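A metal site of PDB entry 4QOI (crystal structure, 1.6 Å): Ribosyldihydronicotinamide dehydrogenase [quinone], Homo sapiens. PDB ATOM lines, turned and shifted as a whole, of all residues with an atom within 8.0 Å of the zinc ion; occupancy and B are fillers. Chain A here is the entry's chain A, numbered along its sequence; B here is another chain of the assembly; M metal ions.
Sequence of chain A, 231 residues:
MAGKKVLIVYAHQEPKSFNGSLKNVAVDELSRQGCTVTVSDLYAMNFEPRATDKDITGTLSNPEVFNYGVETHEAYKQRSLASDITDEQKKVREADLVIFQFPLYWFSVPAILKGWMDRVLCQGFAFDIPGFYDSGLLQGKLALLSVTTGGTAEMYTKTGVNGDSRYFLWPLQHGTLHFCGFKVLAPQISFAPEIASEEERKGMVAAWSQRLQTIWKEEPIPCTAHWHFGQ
O of Gln 173 is in hydrogen-bond range of N of His 178, at 2.8 Å.
A ring nitrogen (NE2) of His 178 sits at hydrogen-bond distance from the side-chain carboxylate of Asp 134 (2.8 Å).
A ring nitrogen (NE2) of His 174 lies within hydrogen-bond range of the side-chain hydroxyl (OH) of Tyr 133 (3.2 Å).
N of Phe 179 lies within hydrogen-bond range of O of His 174.
A ring nitrogen (NE2) of His 174 lies within hydrogen-bond range of the backbone carbonyl oxygen (O) of Val 161 of chain B (3.0 Å).
The side-chain sulfur (SG) of Cys 223 lies close to the backbone carbonyl oxygen (O) of Gln 173, 3.6 Å away.
Three residues have an atom within 4 Å of the zinc ion: His 174, His 178 and Cys 223.
The zinc ion is bound by ND1 of His 178 (2.0 Å), ND1 of His 174 (2.0 Å), O of Cys 223 (2.1 Å) and SG of Cys 223 (2.2 Å).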
ATOM      1  N   TYR A 133     -13.718 -25.273  -5.968  1.00  0.00           N
ATOM      2  CA  TYR A 133     -12.458 -25.721  -6.487  1.00  0.00           C
ATOM      3  C   TYR A 133     -12.138 -24.990  -7.808  1.00  0.00           C
ATOM      4  O   TYR A 133     -12.136 -23.832  -7.788  1.00  0.00           O
ATOM      5  CB  TYR A 133     -12.371 -27.253  -6.545  1.00  0.00           C
ATOM      6  CG  TYR A 133     -12.234 -27.915  -5.182  1.00  0.00           C
ATOM      7  CD1 TYR A 133     -11.213 -27.585  -4.369  1.00  0.00           C
ATOM      8  CD2 TYR A 133     -13.131 -28.859  -4.743  1.00  0.00           C
ATOM      9  CE1 TYR A 133     -11.077 -28.150  -3.137  1.00  0.00           C
ATOM     10  CE2 TYR A 133     -13.006 -29.434  -3.512  1.00  0.00           C
ATOM     11  CZ  TYR A 133     -11.974 -29.064  -2.699  1.00  0.00           C
ATOM     12  OH  TYR A 133     -11.777 -29.601  -1.466  1.00  0.00           O
ATOM     13  N   ASP A 134     -11.904 -25.683  -8.912  1.00  0.00           N
ATOM     14  CA  ASP A 134     -11.531 -24.969 -10.144  1.00  0.00           C
ATOM     15  C   ASP A 134     -12.606 -23.974 -10.643  1.00  0.00           C
ATOM     16  O   ASP A 134     -12.266 -23.029 -11.340  1.00  0.00           O
ATOM     17  CB  ASP A 134     -11.070 -25.927 -11.237  1.00  0.00           C
ATOM     18  CG  ASP A 134      -9.792 -26.693 -10.895  1.00  0.00           C
ATOM     19  OD1 ASP A 134      -9.029 -26.222 -10.005  1.00  0.00           O
ATOM     20  OD2 ASP A 134      -9.491 -27.684 -11.587  1.00  0.00           O
ATOM     21  N   TRP A 170      -2.418 -28.571   3.692  1.00  0.00           N
ATOM     22  CA  TRP A 170      -3.608 -29.096   3.029  1.00  0.00           C
ATOM     23  C   TRP A 170      -4.909 -28.373   3.385  1.00  0.00           C
ATOM     24  O   TRP A 170      -5.591 -27.883   2.474  1.00  0.00           O
ATOM     25  CB  TRP A 170      -3.696 -30.603   3.271  1.00  0.00           C
ATOM     26  CG  TRP A 170      -4.897 -31.272   2.688  1.00  0.00           C
ATOM     27  CD1 TRP A 170      -5.964 -31.792   3.378  1.00  0.00           C
ATOM     28  CD2 TRP A 170      -5.124 -31.591   1.304  1.00  0.00           C
ATOM     29  NE1 TRP A 170      -6.858 -32.371   2.518  1.00  0.00           N
ATOM     30  CE2 TRP A 170      -6.341 -32.307   1.239  1.00  0.00           C
ATOM     31  CE3 TRP A 170      -4.399 -31.359   0.126  1.00  0.00           C
ATOM     32  CZ2 TRP A 170      -6.848 -32.807   0.031  1.00  0.00           C
ATOM     33  CZ3 TRP A 170      -4.929 -31.824  -1.076  1.00  0.00           C
ATOM     34  CH2 TRP A 170      -6.118 -32.571  -1.110  1.00  0.00           C
ATOM     35  N   LEU A 172      -5.471 -25.420   4.463  1.00  0.00           N
ATOM     36  CA  LEU A 172      -5.398 -24.019   4.067  1.00  0.00           C
ATOM     37  C   LEU A 172      -5.339 -23.864   2.538  1.00  0.00           C
ATOM     38  O   LEU A 172      -6.149 -23.150   1.934  1.00  0.00           O
ATOM     39  CB  LEU A 172      -4.162 -23.366   4.698  1.00  0.00           C
ATOM     40  CG  LEU A 172      -4.113 -23.398   6.242  1.00  0.00           C
ATOM     41  CD1 LEU A 172      -2.768 -22.892   6.751  1.00  0.00           C
ATOM     42  CD2 LEU A 172      -5.247 -22.570   6.855  1.00  0.00           C
ATOM     43  N   GLN A 173      -4.345 -24.501   1.908  1.00  0.00           N
ATOM     44  CA  GLN A 173      -4.190 -24.378   0.464  1.00  0.00           C
ATOM     45  C   GLN A 173      -5.315 -25.044  -0.296  1.00  0.00           C
ATOM     46  O   GLN A 173      -5.878 -24.421  -1.222  1.00  0.00           O
ATOM     47  CB  GLN A 173      -2.827 -24.937   0.031  1.00  0.00           C
ATOM     48  CG  GLN A 173      -1.683 -24.050   0.550  1.00  0.00           C
ATOM     49  CD  GLN A 173      -0.289 -24.413   0.024  1.00  0.00           C
ATOM     50  OE1 GLN A 173       0.609 -23.560   0.008  1.00  0.00           O
ATOM     51  NE2 GLN A 173      -0.062 -25.673  -0.398  1.00  0.00           N
ATOM     52  N   HIS A 174      -5.635 -26.283   0.054  1.00  0.00           N
ATOM     53  CA  HIS A 174      -6.641 -27.013  -0.701  1.00  0.00           C
ATOM     54  C   HIS A 174      -8.048 -26.781  -0.203  1.00  0.00           C
ATOM     55  O   HIS A 174      -8.932 -26.378  -0.982  1.00  0.00           O
ATOM     56  CB  HIS A 174      -6.331 -28.526  -0.748  1.00  0.00           C
ATOM     57  CG  HIS A 174      -7.273 -29.281  -1.639  1.00  0.00           C
ATOM     58  ND1 HIS A 174      -7.138 -29.262  -3.016  1.00  0.00           N
ATOM     59  CD2 HIS A 174      -8.324 -30.069  -1.303  1.00  0.00           C
ATOM     60  CE1 HIS A 174      -8.114 -30.041  -3.484  1.00  0.00           C
ATOM     61  NE2 HIS A 174      -8.859 -30.550  -2.478  1.00  0.00           N
ATOM     62  N   GLY A 175      -8.261 -27.036   1.082  1.00  0.00           N
ATOM     63  CA  GLY A 175      -9.584 -26.978   1.671  1.00  0.00           C
ATOM     64  C   GLY A 175     -10.174 -25.590   1.663  1.00  0.00           C
ATOM     65  O   GLY A 175     -11.409 -25.447   1.632  1.00  0.00           O
ATOM     66  N   THR A 176      -9.293 -24.543   1.658  1.00  0.00           N
ATOM     67  CA  THR A 176      -9.780 -23.174   1.722  1.00  0.00           C
ATOM     68  C   THR A 176      -9.503 -22.428   0.436  1.00  0.00           C
ATOM     69  O   THR A 176     -10.441 -22.052  -0.266  1.00  0.00           O
ATOM     70  CB  THR A 176      -9.188 -22.444   2.944  1.00  0.00           C
ATOM     71  OG1 THR A 176      -9.352 -23.226   4.125  1.00  0.00           O
ATOM     72  CG2 THR A 176      -9.854 -21.062   3.157  1.00  0.00           C
ATOM     73  N   LEU A 177      -8.231 -22.168   0.139  1.00  0.00           N
ATOM     74  CA  LEU A 177      -7.906 -21.311  -1.027  1.00  0.00           C
ATOM     75  C   LEU A 177      -8.317 -21.909  -2.365  1.00  0.00           C
ATOM     76  O   LEU A 177      -9.061 -21.274  -3.111  1.00  0.00           O
ATOM     77  CB  LEU A 177      -6.411 -20.932  -1.007  1.00  0.00           C
ATOM     78  CG  LEU A 177      -5.960 -20.219   0.283  1.00  0.00           C
ATOM     79  CD1 LEU A 177      -4.408 -20.069   0.327  1.00  0.00           C
ATOM     80  CD2 LEU A 177      -6.697 -18.885   0.484  1.00  0.00           C
ATOM     81  N   HIS A 178      -7.898 -23.150  -2.644  1.00  0.00           N
ATOM     82  CA  HIS A 178      -8.249 -23.826  -3.901  1.00  0.00           C
ATOM     83  C   HIS A 178      -9.787 -23.981  -3.971  1.00  0.00           C
ATOM     84  O   HIS A 178     -10.368 -23.721  -5.030  1.00  0.00           O
ATOM     85  CB  HIS A 178      -7.548 -25.187  -3.983  1.00  0.00           C
ATOM     86  CG  HIS A 178      -7.664 -25.885  -5.308  1.00  0.00           C
ATOM     87  ND1 HIS A 178      -7.092 -27.137  -5.493  1.00  0.00           N
ATOM     88  CD2 HIS A 178      -8.317 -25.525  -6.461  1.00  0.00           C
ATOM     89  CE1 HIS A 178      -7.371 -27.485  -6.755  1.00  0.00           C
ATOM     90  NE2 HIS A 178      -8.120 -26.566  -7.367  1.00  0.00           N
ATOM     91  N   PHE A 179     -10.423 -24.307  -2.848  1.00  0.00           N
ATOM     92  CA  PHE A 179     -11.882 -24.465  -2.801  1.00  0.00           C
ATOM     93  C   PHE A 179     -12.604 -23.195  -3.298  1.00  0.00           C
ATOM     94  O   PHE A 179     -13.626 -23.299  -3.969  1.00  0.00           O
ATOM     95  CB  PHE A 179     -12.345 -24.859  -1.402  1.00  0.00           C
ATOM     96  CG  PHE A 179     -13.823 -25.183  -1.346  1.00  0.00           C
ATOM     97  CD1 PHE A 179     -14.264 -26.467  -1.603  1.00  0.00           C
ATOM     98  CD2 PHE A 179     -14.754 -24.204  -1.011  1.00  0.00           C
ATOM     99  CE1 PHE A 179     -15.645 -26.772  -1.547  1.00  0.00           C
ATOM    100  CE2 PHE A 179     -16.116 -24.508  -0.944  1.00  0.00           C
ATOM    101  CZ  PHE A 179     -16.550 -25.789  -1.195  1.00  0.00           C
ATOM    102  N   PHE A 182      -8.965 -19.879  -5.859  1.00  0.00           N
ATOM    103  CA  PHE A 182      -7.666 -19.237  -6.012  1.00  0.00           C
ATOM    104  C   PHE A 182      -6.658 -20.199  -6.661  1.00  0.00           C
ATOM    105  O   PHE A 182      -6.737 -21.444  -6.508  1.00  0.00           O
ATOM    106  CB  PHE A 182      -7.049 -18.942  -4.623  1.00  0.00           C
ATOM    107  CG  PHE A 182      -7.576 -17.751  -3.854  1.00  0.00           C
ATOM    108  CD1 PHE A 182      -7.104 -16.468  -4.136  1.00  0.00           C
ATOM    109  CD2 PHE A 182      -8.432 -17.923  -2.769  1.00  0.00           C
ATOM    110  CE1 PHE A 182      -7.507 -15.378  -3.363  1.00  0.00           C
ATOM    111  CE2 PHE A 182      -8.871 -16.826  -2.025  1.00  0.00           C
ATOM    112  CZ  PHE A 182      -8.389 -15.554  -2.326  1.00  0.00           C
ATOM    113  N   VAL A 184      -2.971 -21.173  -6.205  1.00  0.00           N
ATOM    114  CA  VAL A 184      -2.104 -21.111  -5.032  1.00  0.00           C
ATOM    115  C   VAL A 184      -0.640 -21.022  -5.414  1.00  0.00           C
ATOM    116  O   VAL A 184      -0.118 -21.953  -6.025  1.00  0.00           O
ATOM    117  CB  VAL A 184      -2.401 -22.324  -4.117  1.00  0.00           C
ATOM    118  CG1 VAL A 184      -1.505 -22.304  -2.879  1.00  0.00           C
ATOM    119  CG2 VAL A 184      -3.887 -22.367  -3.720  1.00  0.00           C
ATOM    120  N   ILE A 221       1.150 -23.699  -7.776  1.00  0.00           N
ATOM    121  CA  ILE A 221       1.461 -25.114  -7.578  1.00  0.00           C
ATOM    122  C   ILE A 221       0.268 -25.920  -8.091  1.00  0.00           C
ATOM    123  O   ILE A 221      -0.865 -25.388  -8.169  1.00  0.00           O
ATOM    124  CB  ILE A 221       1.681 -25.433  -6.061  1.00  0.00           C
ATOM    125  CG1 ILE A 221       0.364 -25.200  -5.226  1.00  0.00           C
ATOM    126  CG2 ILE A 221       2.889 -24.687  -5.506  1.00  0.00           C
ATOM    127  CD1 ILE A 221       0.279 -25.832  -3.855  1.00  0.00           C
ATOM    128  N   PRO A 222       0.462 -27.219  -8.360  1.00  0.00           N
ATOM    129  CA  PRO A 222      -0.691 -28.082  -8.650  1.00  0.00           C
ATOM    130  C   PRO A 222      -1.252 -28.433  -7.267  1.00  0.00           C
ATOM    131  O   PRO A 222      -0.643 -29.193  -6.524  1.00  0.00           O
ATOM    132  CB  PRO A 222      -0.062 -29.311  -9.338  1.00  0.00           C
ATOM    133  CG  PRO A 222       1.376 -29.327  -8.919  1.00  0.00           C
ATOM    134  CD  PRO A 222       1.741 -27.968  -8.362  1.00  0.00           C
ATOM    135  N   CYS A 223      -2.344 -27.779  -6.859  1.00  0.00           N
ATOM    136  CA  CYS A 223      -2.880 -27.948  -5.511  1.00  0.00           C
ATOM    137  C   CYS A 223      -3.670 -29.259  -5.394  1.00  0.00           C
ATOM    138  O   CYS A 223      -4.913 -29.294  -5.465  1.00  0.00           O
ATOM    139  CB  CYS A 223      -3.700 -26.725  -5.134  1.00  0.00           C
ATOM    140  SG  CYS A 223      -4.237 -26.766  -3.409  1.00  0.00           S
ATOM    141  N   THR A 224      -2.909 -30.386  -5.352  1.00  0.00           N
ATOM    142  CA  THR A 224      -3.484 -31.730  -5.323  1.00  0.00           C
ATOM    143  C   THR A 224      -2.993 -32.508  -4.123  1.00  0.00           C
ATOM    144  O   THR A 224      -1.987 -32.148  -3.515  1.00  0.00           O
ATOM    145  CB  THR A 224      -3.009 -32.482  -6.600  1.00  0.00           C
ATOM    146  OG1 THR A 224      -1.586 -32.587  -6.547  1.00  0.00           O
ATOM    147  CG2 THR A 224      -3.424 -31.762  -7.902  1.00  0.00           C
ATOM    148  N   ALA A 225      -3.658 -33.657  -3.838  1.00  0.00           N
ATOM    149  CA  ALA A 225      -3.213 -34.529  -2.756  1.00  0.00           C
ATOM    150  C   ALA A 225      -1.782 -35.018  -3.067  1.00  0.00           C
ATOM    151  O   ALA A 225      -0.959 -35.079  -2.144  1.00  0.00           O
ATOM    152  CB  ALA A 225      -4.164 -35.720  -2.601  1.00  0.00           C
ATOM    153  N   TRP A 227       0.691 -33.407  -4.633  1.00  0.00           N
ATOM    154  CA  TRP A 227       1.661 -32.360  -4.271  1.00  0.00           C
ATOM    155  C   TRP A 227       1.889 -32.325  -2.754  1.00  0.00           C
ATOM    156  O   TRP A 227       3.030 -32.219  -2.299  1.00  0.00           O
ATOM    157  CB  TRP A 227       1.166 -30.981  -4.759  1.00  0.00           C
ATOM    158  CG  TRP A 227       2.181 -29.875  -4.569  1.00  0.00           C
ATOM    159  CD1 TRP A 227       3.134 -29.489  -5.468  1.00  0.00           C
ATOM    160  CD2 TRP A 227       2.339 -29.031  -3.426  1.00  0.00           C
ATOM    161  NE1 TRP A 227       3.890 -28.464  -4.949  1.00  0.00           N
ATOM    162  CE2 TRP A 227       3.411 -28.153  -3.693  1.00  0.00           C
ATOM    163  CE3 TRP A 227       1.698 -28.941  -2.174  1.00  0.00           C
ATOM    164  CZ2 TRP A 227       3.848 -27.190  -2.785  1.00  0.00           C
ATOM    165  CZ3 TRP A 227       2.129 -27.991  -1.253  1.00  0.00           C
ATOM    166  CH2 TRP A 227       3.194 -27.147  -1.556  1.00  0.00           C
ATOM    167  N   HIS A 228       0.812 -32.452  -1.963  1.00  0.00           N
ATOM    168  CA  HIS A 228       0.944 -32.332  -0.525  1.00  0.00           C
ATOM    169  C   HIS A 228       1.478 -33.572   0.165  1.00  0.00           C
ATOM    170  O   HIS A 228       2.201 -33.445   1.168  1.00  0.00           O
ATOM    171  CB  HIS A 228      -0.407 -31.936   0.118  1.00  0.00           C
ATOM    172  CG  HIS A 228      -0.883 -30.558  -0.225  1.00  0.00           C
ATOM    173  ND1 HIS A 228      -1.528 -30.288  -1.417  1.00  0.00           N
ATOM    174  CD2 HIS A 228      -0.851 -29.427   0.537  1.00  0.00           C
ATOM    175  CE1 HIS A 228      -1.840 -28.992  -1.369  1.00  0.00           C
ATOM    176  NE2 HIS A 228      -1.462 -28.436  -0.211  1.00  0.00           N
ATOM    177  N   VAL B 161     -13.129 -35.192  -4.275  1.00  0.00           N
ATOM    178  CA  VAL B 161     -12.732 -33.771  -4.406  1.00  0.00           C
ATOM    179  C   VAL B 161     -12.023 -33.218  -3.183  1.00  0.00           C
ATOM    180  O   VAL B 161     -11.105 -32.375  -3.301  1.00  0.00           O
ATOM    181  CB  VAL B 161     -13.898 -32.834  -4.834  1.00  0.00           C
ATOM    182  CG1 VAL B 161     -14.212 -32.975  -6.321  1.00  0.00           C
ATOM    183  CG2 VAL B 161     -15.164 -33.050  -3.981  1.00  0.00           C
HETATM  184 ZN    ZN M   1      -5.958 -28.017  -4.114  1.00  0.00          ZN
